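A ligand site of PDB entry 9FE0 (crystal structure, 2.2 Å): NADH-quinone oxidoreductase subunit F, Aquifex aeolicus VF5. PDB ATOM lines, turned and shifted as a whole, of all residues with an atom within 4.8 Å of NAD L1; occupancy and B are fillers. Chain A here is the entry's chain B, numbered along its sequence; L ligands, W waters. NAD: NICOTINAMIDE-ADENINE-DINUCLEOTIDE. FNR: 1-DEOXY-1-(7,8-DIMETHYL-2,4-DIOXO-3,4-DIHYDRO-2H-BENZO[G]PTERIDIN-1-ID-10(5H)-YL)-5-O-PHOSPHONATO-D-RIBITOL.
N of Glu 95 lies within hydrogen-bond range of O4 of FNR L2 (2.9 Å). O2 of FNR L2 sits close to OD1 of Asn 220, at 2.8 Å. N of Ser 96 lies within hydrogen-bond range of O7N of NAD L1, 3.1 Å away. The backbone NH of Glu 97 sits at hydrogen-bond distance from an oxygen (O7N) of NAD L1, at 3.3 Å. The backbone NH of Asn 220 sits at hydrogen-bond distance from an oxygen (O2P) of FNR L2. NZ of Lys 202 lies within salt-bridge range of O2N of NAD L1 (3.2 Å). NZ of Lys 76 is in hydrogen-bond range of O3B of NAD L1, 2.7 Å away. The backbone NH (N) of Glu 185 is in hydrogen-bond range of an oxygen (O2') of FNR L2, at 3.2 Å. The backbone NH of Gly 67 is in hydrogen-bond range of an oxygen (O3P) of FNR L2, at 2.7 Å. O of Gly 68 sits at hydrogen-bond distance from O3D of NAD L1 (3.4 Å). The side-chain amino group (NZ) of Lys 76 lies within salt-bridge range of an oxygen (O1P) of FNR L2, 2.7 Å away. The side-chain carboxylate (OE2) of Glu 185 sits at hydrogen-bond distance from an oxygen (O2B) of NAD L1, 2.5 Å away.
Water W5 lies within hydrogen-bond range of OE2 of Glu 184 (2.7 Å), O1N of NAD L1 (2.7 Å) and N of Gly 394 (3.1 Å). Water W4 bridges the side-chain carboxylate (OE2) of Glu 95 (2.8 Å) and a nitrogen (N7N) of NAD L1 (2.9 Å).
The backbone carbonyl oxygen (O) of Gly 67 sits close to a nitrogen (N1N) of NAD L1, 3.5 Å away. Merely in contact with NAD L1: Tyr 180 (3.1 Å), Glu 95 (3.2 Å), Phe 71 (3.3 Å), Tyr 205 (3.4 Å), Ala 69 (3.4 Å), Phe 79 (3.5 Å), Thr 319 (3.6 Å), Pro 206 (3.7 Å), Leu 297 (3.8 Å) and Val 207 (3.8 Å). Within 4 Å of NAD L1: Gly 67, Gly 68, Ala 69, Phe 71, Lys 76, Phe 79, Glu 95, Ser 96, Glu 97, Tyr 180, Glu 185, Lys 202, Tyr 205, Pro 206, Val 207, Leu 297 and Thr 319. The nearest printed residue that does not touch NAD L1 is Val 218 (4.1 Å).
An oxygen (O2N) of NAD L1 is in hydrogen-bond range of an oxygen (O2') of FNR L2 (2.8 Å).
The side-chain carboxylate (OE2) of Glu 184 lies within salt-bridge range of the side-chain amino group (NZ) of Lys 202, at 3.5 Å. The backbone carbonyl oxygen (O) of Glu 97 sits close to the side-chain hydroxyl (OG1) of Thr 100 (3.3 Å). The side-chain carboxylate (OE2) of Glu 185 is in salt-bridge range of the side-chain amino group (NZ) of Lys 202 (2.9 Å). The side-chain hydroxyl (OH) of Tyr 180 is in hydrogen-bond range of the side-chain carboxylate (OE2) of Glu 97. O of Val 218 is in hydrogen-bond range of NZ of Lys 76 (2.7 Å).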
ATOM      1  N   GLY A  67      -5.173  10.560   9.242  1.00  0.00           N
ATOM      2  CA  GLY A  67      -5.201   9.723   8.053  1.00  0.00           C
ATOM      3  C   GLY A  67      -5.666   8.303   8.368  1.00  0.00           C
ATOM      4  O   GLY A  67      -6.027   7.567   7.455  1.00  0.00           O
ATOM      5  N   GLY A  68      -5.617   7.917   9.653  1.00  0.00           N
ATOM      6  CA  GLY A  68      -6.173   6.640  10.072  1.00  0.00           C
ATOM      7  C   GLY A  68      -5.320   5.923  11.121  1.00  0.00           C
ATOM      8  O   GLY A  68      -5.842   5.156  11.917  1.00  0.00           O
ATOM      9  N   ALA A  69      -4.007   6.169  11.109  1.00  0.00           N
ATOM     10  CA  ALA A  69      -3.097   5.423  11.954  1.00  0.00           C
ATOM     11  C   ALA A  69      -2.888   6.128  13.294  1.00  0.00           C
ATOM     12  O   ALA A  69      -2.394   5.513  14.242  1.00  0.00           O
ATOM     13  CB  ALA A  69      -1.788   5.198  11.236  1.00  0.00           C
ATOM     14  N   PHE A  71      -0.796   8.419  14.260  1.00  0.00           N
ATOM     15  CA  PHE A  71       0.588   8.587  14.700  1.00  0.00           C
ATOM     16  C   PHE A  71       0.813  10.028  15.170  1.00  0.00           C
ATOM     17  O   PHE A  71       0.352  10.983  14.536  1.00  0.00           O
ATOM     18  CB  PHE A  71       1.571   8.236  13.578  1.00  0.00           C
ATOM     19  CG  PHE A  71       2.998   8.090  14.054  1.00  0.00           C
ATOM     20  CD1 PHE A  71       3.459   6.860  14.543  1.00  0.00           C
ATOM     21  CD2 PHE A  71       3.883   9.153  14.015  1.00  0.00           C
ATOM     22  CE1 PHE A  71       4.766   6.732  15.002  1.00  0.00           C
ATOM     23  CE2 PHE A  71       5.193   9.012  14.449  1.00  0.00           C
ATOM     24  CZ  PHE A  71       5.625   7.800  14.950  1.00  0.00           C
ATOM     25  N   LYS A  76       6.525  12.748  14.389  1.00  0.00           N
ATOM     26  CA  LYS A  76       6.838  12.496  13.003  1.00  0.00           C
ATOM     27  C   LYS A  76       7.782  13.578  12.473  1.00  0.00           C
ATOM     28  O   LYS A  76       8.784  13.277  11.829  1.00  0.00           O
ATOM     29  CB  LYS A  76       5.577  12.426  12.140  1.00  0.00           C
ATOM     30  CG  LYS A  76       5.818  11.856  10.745  1.00  0.00           C
ATOM     31  CD  LYS A  76       4.623  11.885   9.803  1.00  0.00           C
ATOM     32  CE  LYS A  76       3.427  11.098  10.252  1.00  0.00           C
ATOM     33  NZ  LYS A  76       2.437  10.913   9.180  1.00  0.00           N
ATOM     34  N   PHE A  79      11.394  13.509  13.738  1.00  0.00           N
ATOM     35  CA  PHE A  79      12.173  12.476  13.072  1.00  0.00           C
ATOM     36  C   PHE A  79      12.748  13.011  11.753  1.00  0.00           C
ATOM     37  O   PHE A  79      13.893  12.750  11.433  1.00  0.00           O
ATOM     38  CB  PHE A  79      11.346  11.212  12.852  1.00  0.00           C
ATOM     39  CG  PHE A  79      11.090  10.310  14.054  1.00  0.00           C
ATOM     40  CD1 PHE A  79      12.002  10.243  15.115  1.00  0.00           C
ATOM     41  CD2 PHE A  79       9.960   9.516  14.122  1.00  0.00           C
ATOM     42  CE1 PHE A  79      11.758   9.399  16.201  1.00  0.00           C
ATOM     43  CE2 PHE A  79       9.728   8.667  15.203  1.00  0.00           C
ATOM     44  CZ  PHE A  79      10.629   8.616  16.239  1.00  0.00           C
ATOM     45  N   GLU A  95      -7.923  10.549   0.120  1.00  0.00           N
ATOM     46  CA  GLU A  95      -9.178  10.108   0.738  1.00  0.00           C
ATOM     47  C   GLU A  95     -10.031   9.215  -0.168  1.00  0.00           C
ATOM     48  O   GLU A  95     -10.879   9.726  -0.919  1.00  0.00           O
ATOM     49  CB  GLU A  95      -9.961  11.347   1.170  1.00  0.00           C
ATOM     50  CG  GLU A  95     -11.304  11.012   1.807  1.00  0.00           C
ATOM     51  CD  GLU A  95     -12.001  12.195   2.426  1.00  0.00           C
ATOM     52  OE1 GLU A  95     -12.576  13.073   1.696  1.00  0.00           O
ATOM     53  OE2 GLU A  95     -11.966  12.210   3.679  1.00  0.00           O
ATOM     54  N   SER A  96      -9.833   7.890  -0.071  1.00  0.00           N
ATOM     55  CA  SER A  96     -10.568   6.952  -0.914  1.00  0.00           C
ATOM     56  C   SER A  96     -11.136   5.744  -0.166  1.00  0.00           C
ATOM     57  O   SER A  96     -11.768   4.896  -0.801  1.00  0.00           O
ATOM     58  CB  SER A  96      -9.726   6.523  -2.093  1.00  0.00           C
ATOM     59  OG  SER A  96      -9.708   7.540  -3.085  1.00  0.00           O
ATOM     60  N   GLU A  97     -10.959   5.686   1.159  1.00  0.00           N
ATOM     61  CA  GLU A  97     -11.569   4.646   1.962  1.00  0.00           C
ATOM     62  C   GLU A  97     -13.095   4.742   1.927  1.00  0.00           C
ATOM     63  O   GLU A  97     -13.635   5.820   2.124  1.00  0.00           O
ATOM     64  CB  GLU A  97     -11.140   4.839   3.422  1.00  0.00           C
ATOM     65  CG  GLU A  97     -11.705   3.803   4.385  1.00  0.00           C
ATOM     66  CD  GLU A  97     -10.843   2.561   4.518  1.00  0.00           C
ATOM     67  OE1 GLU A  97     -10.957   1.853   5.551  1.00  0.00           O
ATOM     68  OE2 GLU A  97     -10.065   2.326   3.545  1.00  0.00           O
ATOM     69  N   THR A 100     -15.557   7.417   3.902  1.00  0.00           N
ATOM     70  CA  THR A 100     -14.717   8.510   4.363  1.00  0.00           C
ATOM     71  C   THR A 100     -14.812   9.692   3.390  1.00  0.00           C
ATOM     72  O   THR A 100     -14.389   9.600   2.240  1.00  0.00           O
ATOM     73  CB  THR A 100     -13.286   8.005   4.554  1.00  0.00           C
ATOM     74  OG1 THR A 100     -13.355   6.787   5.294  1.00  0.00           O
ATOM     75  CG2 THR A 100     -12.426   9.001   5.304  1.00  0.00           C
ATOM     76  N   TYR A 180      -6.858   3.455  -5.185  1.00  0.00           N
ATOM     77  CA  TYR A 180      -6.916   3.553  -3.726  1.00  0.00           C
ATOM     78  C   TYR A 180      -5.520   3.480  -3.106  1.00  0.00           C
ATOM     79  O   TYR A 180      -5.250   4.151  -2.110  1.00  0.00           O
ATOM     80  CB  TYR A 180      -7.796   2.427  -3.192  1.00  0.00           C
ATOM     81  CG  TYR A 180      -7.782   2.121  -1.696  1.00  0.00           C
ATOM     82  CD1 TYR A 180      -8.411   2.952  -0.781  1.00  0.00           C
ATOM     83  CD2 TYR A 180      -7.208   0.958  -1.210  1.00  0.00           C
ATOM     84  CE1 TYR A 180      -8.451   2.644   0.570  1.00  0.00           C
ATOM     85  CE2 TYR A 180      -7.230   0.633   0.142  1.00  0.00           C
ATOM     86  CZ  TYR A 180      -7.858   1.482   1.041  1.00  0.00           C
ATOM     87  OH  TYR A 180      -7.864   1.162   2.368  1.00  0.00           O
ATOM     88  N   GLU A 184      -1.659   5.217   0.155  1.00  0.00           N
ATOM     89  CA  GLU A 184      -0.555   4.700   0.975  1.00  0.00           C
ATOM     90  C   GLU A 184       0.645   5.592   0.711  1.00  0.00           C
ATOM     91  O   GLU A 184       0.968   5.881  -0.443  1.00  0.00           O
ATOM     92  CB  GLU A 184      -0.320   3.213   0.712  1.00  0.00           C
ATOM     93  CG  GLU A 184       0.462   2.503   1.824  1.00  0.00           C
ATOM     94  CD  GLU A 184       1.970   2.655   1.810  1.00  0.00           C
ATOM     95  OE1 GLU A 184       2.533   3.069   0.784  1.00  0.00           O
ATOM     96  OE2 GLU A 184       2.605   2.384   2.861  1.00  0.00           O
ATOM     97  N   GLU A 185       1.280   6.084   1.777  1.00  0.00           N
ATOM     98  CA  GLU A 185       2.225   7.191   1.679  1.00  0.00           C
ATOM     99  C   GLU A 185       3.381   6.880   0.724  1.00  0.00           C
ATOM    100  O   GLU A 185       3.824   7.785   0.027  1.00  0.00           O
ATOM    101  CB  GLU A 185       2.703   7.623   3.059  1.00  0.00           C
ATOM    102  CG  GLU A 185       3.461   6.542   3.827  1.00  0.00           C
ATOM    103  CD  GLU A 185       3.954   6.960   5.199  1.00  0.00           C
ATOM    104  OE1 GLU A 185       3.824   8.150   5.582  1.00  0.00           O
ATOM    105  OE2 GLU A 185       4.502   6.078   5.881  1.00  0.00           O
ATOM    106  N   LYS A 202       8.657  -0.350   4.302  1.00  0.00           N
ATOM    107  CA  LYS A 202       8.988   0.503   5.424  1.00  0.00           C
ATOM    108  C   LYS A 202       9.478  -0.387   6.568  1.00  0.00           C
ATOM    109  O   LYS A 202       8.802  -1.353   6.875  1.00  0.00           O
ATOM    110  CB  LYS A 202       7.747   1.249   5.927  1.00  0.00           C
ATOM    111  CG  LYS A 202       7.007   2.094   4.892  1.00  0.00           C
ATOM    112  CD  LYS A 202       5.492   2.135   5.053  1.00  0.00           C
ATOM    113  CE  LYS A 202       4.994   2.808   6.297  1.00  0.00           C
ATOM    114  NZ  LYS A 202       3.608   3.298   6.133  1.00  0.00           N
ATOM    115  N   TYR A 205      11.025   4.612   6.615  1.00  0.00           N
ATOM    116  CA  TYR A 205       9.840   5.451   6.604  1.00  0.00           C
ATOM    117  C   TYR A 205      10.153   6.717   5.800  1.00  0.00           C
ATOM    118  O   TYR A 205      11.309   7.092   5.639  1.00  0.00           O
ATOM    119  CB  TYR A 205       9.384   5.792   8.030  1.00  0.00           C
ATOM    120  CG  TYR A 205       8.871   4.611   8.856  1.00  0.00           C
ATOM    121  CD1 TYR A 205       7.593   4.113   8.666  1.00  0.00           C
ATOM    122  CD2 TYR A 205       9.664   4.037   9.851  1.00  0.00           C
ATOM    123  CE1 TYR A 205       7.120   3.043   9.414  1.00  0.00           C
ATOM    124  CE2 TYR A 205       9.205   2.960  10.604  1.00  0.00           C
ATOM    125  CZ  TYR A 205       7.931   2.470  10.394  1.00  0.00           C
ATOM    126  OH  TYR A 205       7.473   1.410  11.130  1.00  0.00           O
ATOM    127  N   PRO A 206       9.133   7.410   5.238  1.00  0.00           N
ATOM    128  CA  PRO A 206       9.355   8.602   4.418  1.00  0.00           C
ATOM    129  C   PRO A 206      10.263   9.686   5.007  1.00  0.00           C
ATOM    130  O   PRO A 206      11.029  10.290   4.263  1.00  0.00           O
ATOM    131  CB  PRO A 206       7.925   9.107   4.227  1.00  0.00           C
ATOM    132  CG  PRO A 206       7.109   7.854   4.177  1.00  0.00           C
ATOM    133  CD  PRO A 206       7.716   7.012   5.281  1.00  0.00           C
ATOM    134  N   VAL A 207      10.172   9.887   6.331  1.00  0.00           N
ATOM    135  CA  VAL A 207      10.908  10.946   7.024  1.00  0.00           C
ATOM    136  C   VAL A 207      12.410  10.682   6.937  1.00  0.00           C
ATOM    137  O   VAL A 207      13.204  11.593   7.161  1.00  0.00           O
ATOM    138  CB  VAL A 207      10.485  11.150   8.491  1.00  0.00           C
ATOM    139  CG1 VAL A 207       9.075  11.714   8.598  1.00  0.00           C
ATOM    140  CG2 VAL A 207      10.638   9.884   9.320  1.00  0.00           C
ATOM    141  N   VAL A 218       4.754  13.027   5.219  1.00  0.00           N
ATOM    142  CA  VAL A 218       3.416  12.898   4.691  1.00  0.00           C
ATOM    143  C   VAL A 218       2.432  13.059   5.839  1.00  0.00           C
ATOM    144  O   VAL A 218       2.508  12.334   6.838  1.00  0.00           O
ATOM    145  CB  VAL A 218       3.194  11.542   3.986  1.00  0.00           C
ATOM    146  CG1 VAL A 218       1.822  11.474   3.345  1.00  0.00           C
ATOM    147  CG2 VAL A 218       4.270  11.255   2.942  1.00  0.00           C
ATOM    148  N   ASN A 220      -1.970  13.850   6.625  1.00  0.00           N
ATOM    149  CA  ASN A 220      -3.339  13.884   6.147  1.00  0.00           C
ATOM    150  C   ASN A 220      -3.890  15.319   6.215  1.00  0.00           C
ATOM    151  O   ASN A 220      -3.501  16.078   7.095  1.00  0.00           O
ATOM    152  CB  ASN A 220      -4.165  12.890   6.967  1.00  0.00           C
ATOM    153  CG  ASN A 220      -5.633  12.972   6.624  1.00  0.00           C
ATOM    154  OD1 ASN A 220      -6.062  12.556   5.534  1.00  0.00           O
ATOM    155  ND2 ASN A 220      -6.414  13.520   7.539  1.00  0.00           N
ATOM    156  N   LEU A 297     -12.252  -1.294   7.437  1.00  0.00           N
ATOM    157  CA  LEU A 297     -11.189  -1.687   8.342  1.00  0.00           C
ATOM    158  C   LEU A 297     -11.711  -2.557   9.485  1.00  0.00           C
ATOM    159  O   LEU A 297     -11.159  -3.625   9.746  1.00  0.00           O
ATOM    160  CB  LEU A 297     -10.519  -0.417   8.850  1.00  0.00           C
ATOM    161  CG  LEU A 297      -9.218  -0.589   9.642  1.00  0.00           C
ATOM    162  CD1 LEU A 297      -8.106  -1.016   8.711  1.00  0.00           C
ATOM    163  CD2 LEU A 297      -8.826   0.690  10.366  1.00  0.00           C
ATOM    164  N   GLY A 318      -8.944   5.021  13.994  1.00  0.00           N
ATOM    165  CA  GLY A 318      -9.081   5.100  12.558  1.00  0.00           C
ATOM    166  C   GLY A 318      -9.287   6.525  12.051  1.00  0.00           C
ATOM    167  O   GLY A 318      -8.699   7.479  12.565  1.00  0.00           O
ATOM    168  N   THR A 319     -10.106   6.659  10.993  1.00  0.00           N
ATOM    169  CA  THR A 319     -10.450   7.955  10.447  1.00  0.00           C
ATOM    170  C   THR A 319     -11.697   8.507  11.136  1.00  0.00           C
ATOM    171  O   THR A 319     -12.108   9.613  10.826  1.00  0.00           O
ATOM    172  CB  THR A 319     -10.652   7.854   8.939  1.00  0.00           C
ATOM    173  OG1 THR A 319     -11.571   6.785   8.740  1.00  0.00           O
ATOM    174  CG2 THR A 319      -9.355   7.576   8.200  1.00  0.00           C
ATOM    175  N   GLY A 394      -0.230  -1.885   4.382  1.00  0.00           N
ATOM    176  CA  GLY A 394      -1.356  -2.117   5.275  1.00  0.00           C
ATOM    177  C   GLY A 394      -2.606  -2.665   4.563  1.00  0.00           C
ATOM    178  O   GLY A 394      -3.488  -3.179   5.243  1.00  0.00           O
HETATM  179  PA  NAD L   1       1.509   3.212   9.831  1.00  0.00           P
HETATM  180  O1A NAD L   1       1.149   2.874  11.239  1.00  0.00           O
HETATM  181  O2A NAD L   1       2.422   2.283   9.114  1.00  0.00           O
HETATM  182  O5B NAD L   1       2.158   4.680   9.767  1.00  0.00           O
HETATM  183  C5B NAD L   1       1.374   5.850  10.075  1.00  0.00           C
HETATM  184  C4B NAD L   1       2.216   7.085   9.889  1.00  0.00           C
HETATM  185  O4B NAD L   1       3.229   7.132  10.931  1.00  0.00           O
HETATM  186  C3B NAD L   1       2.990   7.165   8.571  1.00  0.00           C
HETATM  187  O3B NAD L   1       3.116   8.499   8.101  1.00  0.00           O
HETATM  188  C2B NAD L   1       4.348   6.566   8.949  1.00  0.00           C
HETATM  189  O2B NAD L   1       5.360   7.016   8.079  1.00  0.00           O
HETATM  190  C1B NAD L   1       4.519   7.105  10.365  1.00  0.00           C
HETATM  191  N9A NAD L   1       5.395   6.289  11.211  1.00  0.00           N
HETATM  192  C8A NAD L   1       5.060   5.152  11.884  1.00  0.00           C
HETATM  193  N7A NAD L   1       6.044   4.636  12.575  1.00  0.00           N
HETATM  194  C5A NAD L   1       7.107   5.499  12.341  1.00  0.00           C
HETATM  195  C6A NAD L   1       8.447   5.491  12.780  1.00  0.00           C
HETATM  196  N6A NAD L   1       8.958   4.561  13.588  1.00  0.00           N
HETATM  197  N1A NAD L   1       9.257   6.486  12.349  1.00  0.00           N
HETATM  198  C2A NAD L   1       8.737   7.412  11.542  1.00  0.00           C
HETATM  199  N3A NAD L   1       7.500   7.520  11.058  1.00  0.00           N
HETATM  200  C4A NAD L   1       6.726   6.524  11.501  1.00  0.00           C
HETATM  201  O3  NAD L   1       0.173   3.344   8.986  1.00  0.00           O
HETATM  202  PN  NAD L   1      -0.077   3.299   7.399  1.00  0.00           P
HETATM  203  O1N NAD L   1       0.196   1.903   6.925  1.00  0.00           O
HETATM  204  O2N NAD L   1       0.678   4.413   6.736  1.00  0.00           O
HETATM  205  O5D NAD L   1      -1.646   3.608   7.323  1.00  0.00           O
HETATM  206  C5D NAD L   1      -2.688   2.647   7.633  1.00  0.00           C
HETATM  207  C4D NAD L   1      -3.987   3.390   7.895  1.00  0.00           C
HETATM  208  O4D NAD L   1      -4.448   4.041   6.692  1.00  0.00           O
HETATM  209  C3D NAD L   1      -5.182   2.531   8.357  1.00  0.00           C
HETATM  210  O3D NAD L   1      -5.320   2.593   9.765  1.00  0.00           O
HETATM  211  C2D NAD L   1      -6.407   3.128   7.623  1.00  0.00           C
HETATM  212  O2D NAD L   1      -7.432   3.625   8.452  1.00  0.00           O
HETATM  213  C1D NAD L   1      -5.820   4.355   6.906  1.00  0.00           C
HETATM  214  N1N NAD L   1      -6.490   4.673   5.621  1.00  0.00           N
HETATM  215  C2N NAD L   1      -7.111   5.901   5.441  1.00  0.00           C
HETATM  216  C3N NAD L   1      -7.743   6.184   4.232  1.00  0.00           C
HETATM  217  C7N NAD L   1      -8.410   7.519   3.986  1.00  0.00           C
HETATM  218  O7N NAD L   1      -9.024   7.712   2.920  1.00  0.00           O
HETATM  219  N7N NAD L   1      -8.302   8.458   4.912  1.00  0.00           N
HETATM  220  C4N NAD L   1      -7.740   5.238   3.221  1.00  0.00           C
HETATM  221  C5N NAD L   1      -7.130   4.013   3.415  1.00  0.00           C
HETATM  222  C6N NAD L   1      -6.513   3.737   4.618  1.00  0.00           C
HETATM  223  C9A FNR L   2      -3.461   5.010   3.721  1.00  0.00           C
HETATM  224  N10 FNR L   2      -3.325   6.252   4.398  1.00  0.00           N
HETATM  225  CAA FNR L   2      -4.048   7.337   3.942  1.00  0.00           C
HETATM  226  N1  FNR L   2      -3.866   8.552   4.557  1.00  0.00           N
HETATM  227  C2  FNR L   2      -4.436   9.717   4.103  1.00  0.00           C
HETATM  228  O2  FNR L   2      -4.150  10.819   4.575  1.00  0.00           O
HETATM  229  N3  FNR L   2      -5.314   9.587   3.057  1.00  0.00           N
HETATM  230  C4  FNR L   2      -5.598   8.429   2.366  1.00  0.00           C
HETATM  231  O4  FNR L   2      -6.370   8.490   1.405  1.00  0.00           O
HETATM  232  C4A FNR L   2      -4.901   7.264   2.862  1.00  0.00           C
HETATM  233  N5  FNR L   2      -5.020   6.073   2.215  1.00  0.00           N
HETATM  234  C5A FNR L   2      -4.303   4.952   2.610  1.00  0.00           C
HETATM  235  C6  FNR L   2      -4.438   3.751   1.911  1.00  0.00           C
HETATM  236  C7  FNR L   2      -3.753   2.606   2.308  1.00  0.00           C
HETATM  237  C7M FNR L   2      -3.893   1.334   1.518  1.00  0.00           C
HETATM  238  C8  FNR L   2      -2.909   2.668   3.442  1.00  0.00           C
HETATM  239  C8M FNR L   2      -2.211   1.431   3.951  1.00  0.00           C
HETATM  240  C9  FNR L   2      -2.764   3.866   4.126  1.00  0.00           C
HETATM  241  C1' FNR L   2      -2.392   6.385   5.526  1.00  0.00           C
HETATM  242  C2' FNR L   2      -1.078   6.944   4.987  1.00  0.00           C
HETATM  243  O2' FNR L   2      -0.268   5.862   4.524  1.00  0.00           O
HETATM  244  C3' FNR L   2      -0.358   7.711   6.100  1.00  0.00           C
HETATM  245  O3' FNR L   2      -0.439   6.965   7.306  1.00  0.00           O
HETATM  246  C4' FNR L   2      -0.917   9.108   6.363  1.00  0.00           C
HETATM  247  O4' FNR L   2      -1.179   9.829   5.146  1.00  0.00           O
HETATM  248  C5' FNR L   2       0.001   9.884   7.286  1.00  0.00           C
HETATM  249  O5' FNR L   2      -0.654  11.117   7.682  1.00  0.00           O
HETATM  250  P   FNR L   2      -1.138  11.356   9.207  1.00  0.00           P
HETATM  251  O1P FNR L   2      -0.041  10.867  10.131  1.00  0.00           O
HETATM  252  O2P FNR L   2      -1.334  12.861   9.272  1.00  0.00           O
HETATM  253  O3P FNR L   2      -2.431  10.584   9.355  1.00  0.00           O
HETATM  254  O   HOH W   1      -6.339   0.532   5.083  1.00  0.00           O
HETATM  255  O   HOH W   2      11.898   6.388  12.820  1.00  0.00           O
HETATM  256  O   HOH W   3      -0.837   1.554  11.987  1.00  0.00           O
HETATM  257  O   HOH W   4      -9.828  10.911   4.980  1.00  0.00           O
HETATM  258  O   HOH W   5       1.315   0.831   4.654  1.00  0.00           O
